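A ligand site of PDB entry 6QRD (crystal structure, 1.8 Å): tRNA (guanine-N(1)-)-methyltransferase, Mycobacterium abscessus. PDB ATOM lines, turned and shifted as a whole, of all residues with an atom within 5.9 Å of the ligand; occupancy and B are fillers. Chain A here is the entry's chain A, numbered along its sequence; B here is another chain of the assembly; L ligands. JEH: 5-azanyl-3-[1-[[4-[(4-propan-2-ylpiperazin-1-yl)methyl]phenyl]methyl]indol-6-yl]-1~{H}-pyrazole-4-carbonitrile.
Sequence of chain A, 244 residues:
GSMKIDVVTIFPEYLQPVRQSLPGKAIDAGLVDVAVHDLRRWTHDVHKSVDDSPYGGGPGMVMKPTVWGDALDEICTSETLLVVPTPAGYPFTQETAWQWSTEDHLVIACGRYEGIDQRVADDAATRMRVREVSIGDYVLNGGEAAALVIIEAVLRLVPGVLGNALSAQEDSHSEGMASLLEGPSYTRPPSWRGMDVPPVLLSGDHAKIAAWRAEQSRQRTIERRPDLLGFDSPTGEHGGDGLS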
ATOM      1  N   PRO A  85      33.381 -22.173  26.826  1.00  0.00           N
ATOM      2  CA  PRO A  85      32.859 -20.965  26.186  1.00  0.00           C
ATOM      3  C   PRO A  85      31.546 -20.527  26.825  1.00  0.00           C
ATOM      4  O   PRO A  85      30.715 -21.343  27.193  1.00  0.00           O
ATOM      5  CB  PRO A  85      32.642 -21.406  24.743  1.00  0.00           C
ATOM      6  CG  PRO A  85      33.673 -22.472  24.534  1.00  0.00           C
ATOM      7  CD  PRO A  85      33.656 -23.234  25.850  1.00  0.00           C
ATOM      8  N   THR A  86      31.377 -19.217  26.951  1.00  0.00           N
ATOM      9  CA  THR A  86      30.158 -18.662  27.533  1.00  0.00           C
ATOM     10  C   THR A  86      30.111 -17.185  27.204  1.00  0.00           C
ATOM     11  O   THR A  86      31.132 -16.519  27.196  1.00  0.00           O
ATOM     12  CB  THR A  86      30.092 -18.863  29.082  1.00  0.00           C
ATOM     13  OG1 THR A  86      29.072 -18.006  29.630  1.00  0.00           O
ATOM     14  CG2 THR A  86      31.426 -18.577  29.745  1.00  0.00           C
ATOM     15  N   PRO A  87      28.905 -16.669  26.918  1.00  0.00           N
ATOM     16  CA  PRO A  87      28.836 -15.232  26.635  1.00  0.00           C
ATOM     17  C   PRO A  87      29.169 -14.401  27.876  1.00  0.00           C
ATOM     18  O   PRO A  87      29.439 -13.210  27.740  1.00  0.00           O
ATOM     19  CB  PRO A  87      27.389 -15.022  26.182  1.00  0.00           C
ATOM     20  CG  PRO A  87      26.637 -16.181  26.633  1.00  0.00           C
ATOM     21  CD  PRO A  87      27.591 -17.328  26.859  1.00  0.00           C
ATOM     22  N   CYS A 110      31.332 -27.548  25.192  1.00  0.00           N
ATOM     23  CA  CYS A 110      30.429 -26.706  24.417  1.00  0.00           C
ATOM     24  C   CYS A 110      29.011 -26.785  24.933  1.00  0.00           C
ATOM     25  O   CYS A 110      28.384 -27.841  24.881  1.00  0.00           O
ATOM     26  CB  CYS A 110      30.456 -27.112  22.943  1.00  0.00           C
ATOM     27  SG  CYS A 110      32.059 -26.915  22.212  1.00  0.00           S
ATOM     28  N   GLY A 111      28.495 -25.652  25.426  1.00  0.00           N
ATOM     29  CA  GLY A 111      27.119 -25.580  25.852  1.00  0.00           C
ATOM     30  C   GLY A 111      26.170 -25.240  24.720  1.00  0.00           C
ATOM     31  O   GLY A 111      26.569 -24.791  23.631  1.00  0.00           O
ATOM     32  N   ARG A 112      24.889 -25.485  24.993  1.00  0.00           N
ATOM     33  CA  ARG A 112      23.796 -25.044  24.139  1.00  0.00           C
ATOM     34  C   ARG A 112      22.677 -24.536  25.066  1.00  0.00           C
ATOM     35  O   ARG A 112      22.856 -24.487  26.277  1.00  0.00           O
ATOM     36  CB  ARG A 112      23.305 -26.174  23.218  1.00  0.00           C
ATOM     37  CG  ARG A 112      24.212 -26.441  22.009  1.00  0.00           C
ATOM     38  CD  ARG A 112      23.753 -25.569  20.820  1.00  0.00           C
ATOM     39  NE  ARG A 112      24.834 -25.301  19.865  1.00  0.00           N
ATOM     40  CZ  ARG A 112      24.630 -24.781  18.668  1.00  0.00           C
ATOM     41  NH1 ARG A 112      23.396 -24.497  18.262  1.00  0.00           N
ATOM     42  NH2 ARG A 112      25.664 -24.559  17.860  1.00  0.00           N
ATOM     43  N   TYR A 113      21.539 -24.135  24.476  1.00  0.00           N
ATOM     44  CA  TYR A 113      20.454 -23.547  25.264  1.00  0.00           C
ATOM     45  C   TYR A 113      20.933 -22.334  26.056  1.00  0.00           C
ATOM     46  O   TYR A 113      21.634 -21.473  25.506  1.00  0.00           O
ATOM     47  CB  TYR A 113      19.838 -24.611  26.192  1.00  0.00           C
ATOM     48  CG  TYR A 113      19.489 -25.878  25.457  1.00  0.00           C
ATOM     49  CD1 TYR A 113      18.349 -25.956  24.665  1.00  0.00           C
ATOM     50  CD2 TYR A 113      20.289 -27.008  25.555  1.00  0.00           C
ATOM     51  CE1 TYR A 113      18.016 -27.109  23.980  1.00  0.00           C
ATOM     52  CE2 TYR A 113      19.968 -28.173  24.866  1.00  0.00           C
ATOM     53  CZ  TYR A 113      18.834 -28.226  24.090  1.00  0.00           C
ATOM     54  OH  TYR A 113      18.508 -29.377  23.417  1.00  0.00           O
ATOM     55  N   GLU A 114      20.590 -22.228  27.332  1.00  0.00           N
ATOM     56  CA  GLU A 114      21.019 -21.084  28.128  1.00  0.00           C
ATOM     57  C   GLU A 114      22.412 -21.271  28.711  1.00  0.00           C
ATOM     58  O   GLU A 114      22.982 -20.357  29.291  1.00  0.00           O
ATOM     59  CB  GLU A 114      20.028 -20.801  29.259  1.00  0.00           C
ATOM     60  CG  GLU A 114      18.618 -20.517  28.776  1.00  0.00           C
ATOM     61  CD  GLU A 114      18.535 -19.248  27.947  1.00  0.00           C
ATOM     62  OE1 GLU A 114      18.488 -19.340  26.706  1.00  0.00           O
ATOM     63  OE2 GLU A 114      18.528 -18.161  28.551  1.00  0.00           O
ATOM     64  N   GLY A 115      22.984 -22.466  28.533  1.00  0.00           N
ATOM     65  CA  GLY A 115      24.299 -22.764  29.069  1.00  0.00           C
ATOM     66  C   GLY A 115      24.279 -23.980  29.975  1.00  0.00           C
ATOM     67  O   GLY A 115      23.308 -24.728  29.993  1.00  0.00           O
ATOM     68  N   ILE A 116      25.354 -24.159  30.717  1.00  0.00           N
ATOM     69  CA  ILE A 116      25.559 -25.341  31.546  1.00  0.00           C
ATOM     70  C   ILE A 116      25.333 -24.984  32.992  1.00  0.00           C
ATOM     71  O   ILE A 116      25.788 -23.921  33.443  1.00  0.00           O
ATOM     72  CB  ILE A 116      26.966 -25.902  31.364  1.00  0.00           C
ATOM     73  CG1 ILE A 116      27.231 -26.187  29.878  1.00  0.00           C
ATOM     74  CG2 ILE A 116      27.189 -27.183  32.210  1.00  0.00           C
ATOM     75  CD1 ILE A 116      28.682 -26.570  29.590  1.00  0.00           C
ATOM     76  N   VAL A 133      35.354 -18.479  29.125  1.00  0.00           N
ATOM     77  CA  VAL A 133      35.805 -17.419  28.240  1.00  0.00           C
ATOM     78  C   VAL A 133      34.779 -17.104  27.169  1.00  0.00           C
ATOM     79  O   VAL A 133      33.961 -17.940  26.835  1.00  0.00           O
ATOM     80  CB  VAL A 133      37.161 -17.759  27.546  1.00  0.00           C
ATOM     81  CG1 VAL A 133      38.276 -17.903  28.577  1.00  0.00           C
ATOM     82  CG2 VAL A 133      37.049 -19.033  26.692  1.00  0.00           C
ATOM     83  N   SER A 134      34.859 -15.885  26.638  1.00  0.00           N
ATOM     84  CA  SER A 134      34.018 -15.453  25.523  1.00  0.00           C
ATOM     85  C   SER A 134      34.887 -14.996  24.372  1.00  0.00           C
ATOM     86  O   SER A 134      35.866 -14.282  24.607  1.00  0.00           O
ATOM     87  CB  SER A 134      33.090 -14.323  25.933  1.00  0.00           C
ATOM     88  OG  SER A 134      32.486 -13.719  24.804  1.00  0.00           O
ATOM     89  N   ILE A 135      34.524 -15.352  23.135  1.00  0.00           N
ATOM     90  CA  ILE A 135      35.349 -14.952  21.997  1.00  0.00           C
ATOM     91  C   ILE A 135      34.986 -13.583  21.412  1.00  0.00           C
ATOM     92  O   ILE A 135      35.675 -13.089  20.524  1.00  0.00           O
ATOM     93  CB  ILE A 135      35.305 -15.998  20.852  1.00  0.00           C
ATOM     94  CG1 ILE A 135      33.880 -16.173  20.339  1.00  0.00           C
ATOM     95  CG2 ILE A 135      35.952 -17.330  21.288  1.00  0.00           C
ATOM     96  CD1 ILE A 135      33.828 -16.761  18.909  1.00  0.00           C
ATOM     97  N   GLY A 136      33.946 -12.937  21.933  1.00  0.00           N
ATOM     98  CA  GLY A 136      33.608 -11.606  21.458  1.00  0.00           C
ATOM     99  C   GLY A 136      32.271 -11.120  21.942  1.00  0.00           C
ATOM    100  O   GLY A 136      31.502 -11.862  22.552  1.00  0.00           O
ATOM    101  N   ASP A 137      31.975  -9.855  21.633  1.00  0.00           N
ATOM    102  CA  ASP A 137      30.756  -9.259  22.172  1.00  0.00           C
ATOM    103  C   ASP A 137      29.572  -9.360  21.226  1.00  0.00           C
ATOM    104  O   ASP A 137      29.098  -8.353  20.701  1.00  0.00           O
ATOM    105  CB  ASP A 137      31.008  -7.796  22.539  1.00  0.00           C
ATOM    106  CG  ASP A 137      31.931  -7.666  23.740  1.00  0.00           C
ATOM    107  OD1 ASP A 137      32.007  -8.625  24.534  1.00  0.00           O
ATOM    108  OD2 ASP A 137      32.573  -6.607  23.900  1.00  0.00           O
ATOM    109  N   TYR A 138      29.119 -10.590  21.028  1.00  0.00           N
ATOM    110  CA  TYR A 138      27.984 -10.924  20.193  1.00  0.00           C
ATOM    111  C   TYR A 138      27.478 -12.215  20.781  1.00  0.00           C
ATOM    112  O   TYR A 138      28.212 -12.864  21.519  1.00  0.00           O
ATOM    113  CB  TYR A 138      28.365 -11.095  18.731  1.00  0.00           C
ATOM    114  CG  TYR A 138      29.731 -11.716  18.553  1.00  0.00           C
ATOM    115  CD1 TYR A 138      29.922 -13.084  18.754  1.00  0.00           C
ATOM    116  CD2 TYR A 138      30.843 -10.926  18.253  1.00  0.00           C
ATOM    117  CE1 TYR A 138      31.182 -13.659  18.623  1.00  0.00           C
ATOM    118  CE2 TYR A 138      32.107 -11.484  18.107  1.00  0.00           C
ATOM    119  CZ  TYR A 138      32.272 -12.846  18.290  1.00  0.00           C
ATOM    120  OH  TYR A 138      33.528 -13.396  18.173  1.00  0.00           O
ATOM    121  N   VAL A 139      26.267 -12.601  20.417  1.00  0.00           N
ATOM    122  CA  VAL A 139      25.637 -13.776  20.998  1.00  0.00           C
ATOM    123  C   VAL A 139      25.528 -14.878  19.955  1.00  0.00           C
ATOM    124  O   VAL A 139      25.081 -14.657  18.843  1.00  0.00           O
ATOM    125  CB  VAL A 139      24.246 -13.419  21.541  1.00  0.00           C
ATOM    126  CG1 VAL A 139      23.587 -14.646  22.159  1.00  0.00           C
ATOM    127  CG2 VAL A 139      24.353 -12.273  22.551  1.00  0.00           C
ATOM    128  N   LEU A 140      25.969 -16.080  20.339  1.00  0.00           N
ATOM    129  CA  LEU A 140      25.896 -17.254  19.482  1.00  0.00           C
ATOM    130  C   LEU A 140      24.819 -18.205  20.021  1.00  0.00           C
ATOM    131  O   LEU A 140      24.231 -17.937  21.068  1.00  0.00           O
ATOM    132  CB  LEU A 140      27.241 -17.956  19.435  1.00  0.00           C
ATOM    133  CG  LEU A 140      28.459 -17.119  19.002  1.00  0.00           C
ATOM    134  CD1 LEU A 140      29.746 -17.879  19.230  1.00  0.00           C
ATOM    135  CD2 LEU A 140      28.337 -16.738  17.531  1.00  0.00           C
ATOM    136  N   ASN A 141      24.554 -19.295  19.307  1.00  0.00           N
ATOM    137  CA  ASN A 141      23.587 -20.297  19.781  1.00  0.00           C
ATOM    138  C   ASN A 141      24.180 -21.281  20.776  1.00  0.00           C
ATOM    139  O   ASN A 141      23.460 -22.003  21.478  1.00  0.00           O
ATOM    140  CB  ASN A 141      23.008 -21.080  18.614  1.00  0.00           C
ATOM    141  CG  ASN A 141      22.083 -20.264  17.765  1.00  0.00           C
ATOM    142  OD1 ASN A 141      21.278 -19.485  18.282  1.00  0.00           O
ATOM    143  ND2 ASN A 141      22.198 -20.421  16.454  1.00  0.00           N
ATOM    144  N   GLY A 142      25.510 -21.334  20.822  1.00  0.00           N
ATOM    145  CA  GLY A 142      26.162 -22.325  21.665  1.00  0.00           C
ATOM    146  C   GLY A 142      27.659 -22.191  21.527  1.00  0.00           C
ATOM    147  O   GLY A 142      28.159 -21.306  20.825  1.00  0.00           O
ATOM    148  N   GLY A 143      28.389 -23.087  22.176  1.00  0.00           N
ATOM    149  CA  GLY A 143      29.830 -22.951  22.257  1.00  0.00           C
ATOM    150  C   GLY A 143      30.636 -23.500  21.102  1.00  0.00           C
ATOM    151  O   GLY A 143      31.848 -23.310  21.068  1.00  0.00           O
ATOM    152  N   ALA A 146      32.576 -20.999  18.985  1.00  0.00           N
ATOM    153  CA  ALA A 146      33.629 -20.461  19.844  1.00  0.00           C
ATOM    154  C   ALA A 146      34.777 -21.450  19.944  1.00  0.00           C
ATOM    155  O   ALA A 146      35.940 -21.069  19.926  1.00  0.00           O
ATOM    156  CB  ALA A 146      33.076 -20.123  21.243  1.00  0.00           C
ATOM    157  N   ILE A 150      38.670 -20.826  19.059  1.00  0.00           N
ATOM    158  CA  ILE A 150      39.701 -21.076  20.063  1.00  0.00           C
ATOM    159  C   ILE A 150      40.729 -22.094  19.576  1.00  0.00           C
ATOM    160  O   ILE A 150      41.949 -21.895  19.713  1.00  0.00           O
ATOM    161  CB  ILE A 150      39.068 -21.554  21.385  1.00  0.00           C
ATOM    162  CG1 ILE A 150      38.316 -20.396  22.035  1.00  0.00           C
ATOM    163  CG2 ILE A 150      40.129 -22.105  22.332  1.00  0.00           C
ATOM    164  CD1 ILE A 150      37.336 -20.799  23.134  1.00  0.00           C
ATOM    165  N   ARG B 156      20.483 -15.806  13.958  1.00  0.00           N
ATOM    166  CA  ARG B 156      19.568 -16.023  15.071  1.00  0.00           C
ATOM    167  C   ARG B 156      18.718 -14.779  15.367  1.00  0.00           C
ATOM    168  O   ARG B 156      17.760 -14.837  16.144  1.00  0.00           O
ATOM    169  CB  ARG B 156      20.336 -16.494  16.315  1.00  0.00           C
ATOM    170  CG  ARG B 156      21.397 -15.564  16.827  1.00  0.00           C
ATOM    171  CD  ARG B 156      22.175 -16.235  17.964  1.00  0.00           C
ATOM    172  NE  ARG B 156      21.365 -16.480  19.153  1.00  0.00           N
ATOM    173  CZ  ARG B 156      20.978 -15.525  20.009  1.00  0.00           C
ATOM    174  NH1 ARG B 156      21.279 -14.253  19.787  1.00  0.00           N
ATOM    175  NH2 ARG B 156      20.254 -15.845  21.068  1.00  0.00           N
ATOM    176  N   SER B 179      25.355  -5.522  27.262  1.00  0.00           N
ATOM    177  CA  SER B 179      25.093  -4.546  28.315  1.00  0.00           C
ATOM    178  C   SER B 179      25.639  -5.025  29.664  1.00  0.00           C
ATOM    179  O   SER B 179      26.474  -4.351  30.275  1.00  0.00           O
ATOM    180  CB  SER B 179      23.593  -4.273  28.437  1.00  0.00           C
ATOM    181  OG  SER B 179      23.004  -4.075  27.157  1.00  0.00           O
ATOM    182  N   LEU B 180      25.169  -6.178  30.100  1.00  0.00           N
ATOM    183  CA  LEU B 180      25.649  -6.829  31.315  1.00  0.00           C
ATOM    184  C   LEU B 180      25.808  -8.308  31.037  1.00  0.00           C
ATOM    185  O   LEU B 180      25.157  -8.830  30.138  1.00  0.00           O
ATOM    186  CB  LEU B 180      24.673  -6.621  32.478  1.00  0.00           C
ATOM    187  CG  LEU B 180      24.541  -5.205  33.022  1.00  0.00           C
ATOM    188  CD1 LEU B 180      23.258  -5.082  33.809  1.00  0.00           C
ATOM    189  CD2 LEU B 180      25.741  -4.867  33.883  1.00  0.00           C
ATOM    190  N   LEU B 181      26.650  -8.996  31.801  1.00  0.00           N
ATOM    191  CA  LEU B 181      26.861 -10.429  31.599  1.00  0.00           C
ATOM    192  C   LEU B 181      25.798 -11.226  32.317  1.00  0.00           C
ATOM    193  O   LEU B 181      25.390 -10.870  33.420  1.00  0.00           O
ATOM    194  CB  LEU B 181      28.243 -10.856  32.078  1.00  0.00           C
ATOM    195  CG  LEU B 181      29.459 -10.156  31.498  1.00  0.00           C
ATOM    196  CD1 LEU B 181      30.737 -10.770  32.038  1.00  0.00           C
ATOM    197  CD2 LEU B 181      29.441 -10.182  29.972  1.00  0.00           C
ATOM    198  N   GLU B 182      25.343 -12.316  31.703  1.00  0.00           N
ATOM    199  CA  GLU B 182      24.411 -13.205  32.359  1.00  0.00           C
ATOM    200  C   GLU B 182      25.041 -13.848  33.589  1.00  0.00           C
ATOM    201  O   GLU B 182      26.219 -14.229  33.569  1.00  0.00           O
ATOM    202  CB  GLU B 182      23.927 -14.301  31.410  1.00  0.00           C
ATOM    203  CG  GLU B 182      22.664 -13.961  30.665  1.00  0.00           C
ATOM    204  CD  GLU B 182      21.528 -13.526  31.583  1.00  0.00           C
ATOM    205  OE1 GLU B 182      21.012 -12.402  31.379  1.00  0.00           O
ATOM    206  OE2 GLU B 182      21.168 -14.296  32.495  1.00  0.00           O
HETATM  207  C10 JEH L   1      26.778 -18.858  23.683  1.00  0.00           C
HETATM  208  C13 JEH L   1      28.436 -20.809  24.858  1.00  0.00           C
HETATM  209  C15 JEH L   1      26.122 -22.003  25.330  1.00  0.00           C
HETATM  210  C20 JEH L   1      23.552 -18.472  26.147  1.00  0.00           C
HETATM  211  C21 JEH L   1      23.103 -17.372  26.909  1.00  0.00           C
HETATM  212  C22 JEH L   1      22.373 -16.346  26.292  1.00  0.00           C
HETATM  213  C26 JEH L   1      22.047 -12.606  25.924  1.00  0.00           C
HETATM  214  C28 JEH L   1      23.232 -11.925  27.684  1.00  0.00           C
HETATM  215  N01 JEH L   1      31.070 -14.749  22.349  1.00  0.00           N
HETATM  216  C02 JEH L   1      29.964 -15.615  22.584  1.00  0.00           C
HETATM  217  N03 JEH L   1      28.651 -15.344  22.331  1.00  0.00           N
HETATM  218  N04 JEH L   1      27.932 -16.434  22.688  1.00  0.00           N
HETATM  219  C05 JEH L   1      28.738 -17.404  23.120  1.00  0.00           C
HETATM  220  C06 JEH L   1      30.032 -16.904  23.106  1.00  0.00           C
HETATM  221  C07 JEH L   1      31.336 -17.562  23.505  1.00  0.00           C
HETATM  222  N08 JEH L   1      32.336 -18.020  23.787  1.00  0.00           N
HETATM  223  C09 JEH L   1      28.179 -18.720  23.679  1.00  0.00           C
HETATM  224  C11 JEH L   1      26.199 -20.035  24.266  1.00  0.00           C
HETATM  225  C12 JEH L   1      27.019 -20.981  24.845  1.00  0.00           C
HETATM  226  C14 JEH L   1      29.011 -19.659  24.290  1.00  0.00           C
HETATM  227  C16 JEH L   1      24.812 -21.612  25.017  1.00  0.00           C
HETATM  228  N17 JEH L   1      24.876 -20.436  24.386  1.00  0.00           N
HETATM  229  C18 JEH L   1      23.731 -19.716  23.886  1.00  0.00           C
HETATM  230  C19 JEH L   1      23.269 -18.534  24.774  1.00  0.00           C
HETATM  231  C23 JEH L   1      21.906 -15.118  27.157  1.00  0.00           C
HETATM  232  N24 JEH L   1      20.839 -14.480  26.803  1.00  0.00           N
HETATM  233  C25 JEH L   1      20.967 -13.643  25.741  1.00  0.00           C
HETATM  234  N27 JEH L   1      22.051 -11.986  27.132  1.00  0.00           N
HETATM  235  C29 JEH L   1      23.361 -10.607  28.425  1.00  0.00           C
HETATM  236  C30 JEH L   1      24.409 -12.169  26.751  1.00  0.00           C
HETATM  237  C31 JEH L   1      21.144 -12.410  28.064  1.00  0.00           C
HETATM  238  C32 JEH L   1      20.399 -13.726  27.843  1.00  0.00           C
HETATM  239  C33 JEH L   1      22.114 -16.422  24.908  1.00  0.00           C
HETATM  240  C34 JEH L   1      22.561 -17.520  24.155  1.00  0.00           C
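A nitrogen (N08) of the ligand lies close to the backbone carbonyl oxygen (O) of Val 133 (3.5 Å). Pro 85 touches the ligand (O to C13, 3.3 Å). Thr 86 touches the ligand. Pro 87 touches the ligand (CD to C09, 3.5 Å). C of Gly 111 touches C15 of the ligand (3.3 Å). Arg 112 touches the ligand (C to C16, 3.6 Å). Tyr 113 touches the ligand. Glu 114 touches the ligand (O to C20, 3.7 Å). Ile 135 touches the ligand (N to N08, 3.5 Å). Val 139 touches the ligand. Asn 141 touches the ligand (O to C18, 3.3 Å). CA of Gly 142 touches C11 of the ligand, 3.5 Å away. N of Gly 143 touches C13 of the ligand (3.5 Å). Ala 146 touches the ligand (CB to N08, 3.4 Å). Leu 180 of chain B touches the ligand (O to C29, 3.1 Å). Glu 182 of chain B touches the ligand. Hydrophobic or aromatic side chains that line the ligand: Pro 85, Pro 87, Ile 135, Tyr 138, Val 139, Leu 140 and Ala 146. Of the 28 residues printed, 20 come within 4 Å of the ligand.
The side-chain amide oxygen (OD1) of Asn 141 lies within hydrogen-bond range of the guanidinium group (NE) of Arg 156 of chain B, at 3.1 Å. OG of Ser 134 is in hydrogen-bond range of O of Gly 136 (3.1 Å). The side-chain hydroxyl of Tyr 138 sits at hydrogen-bond distance from the backbone carbonyl oxygen of Ile 135 (3.2 Å). The backbone carbonyl oxygen of Val 133 sits at hydrogen-bond distance from the backbone NH of Thr 86 (2.9 Å). N of Gly 143 lies within hydrogen-bond range of O of Gly 111, at 2.9 Å. The side-chain sulfur of Cys 110 sits at hydrogen-bond distance from the backbone carbonyl oxygen of Gly 143.
A nitrogen (N01) of the ligand is in hydrogen-bond range of the backbone carbonyl oxygen of Gly 136 (2.9 Å). The side-chain hydroxyl (OG) of Ser 134 sits at hydrogen-bond distance from a nitrogen (N01) of the ligand, at 3.0 Å. N of Leu 140 is in hydrogen-bond range of N04 of the ligand (3.1 Å). O of Tyr 138 is in hydrogen-bond range of N03 of the ligand, at 2.6 Å.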
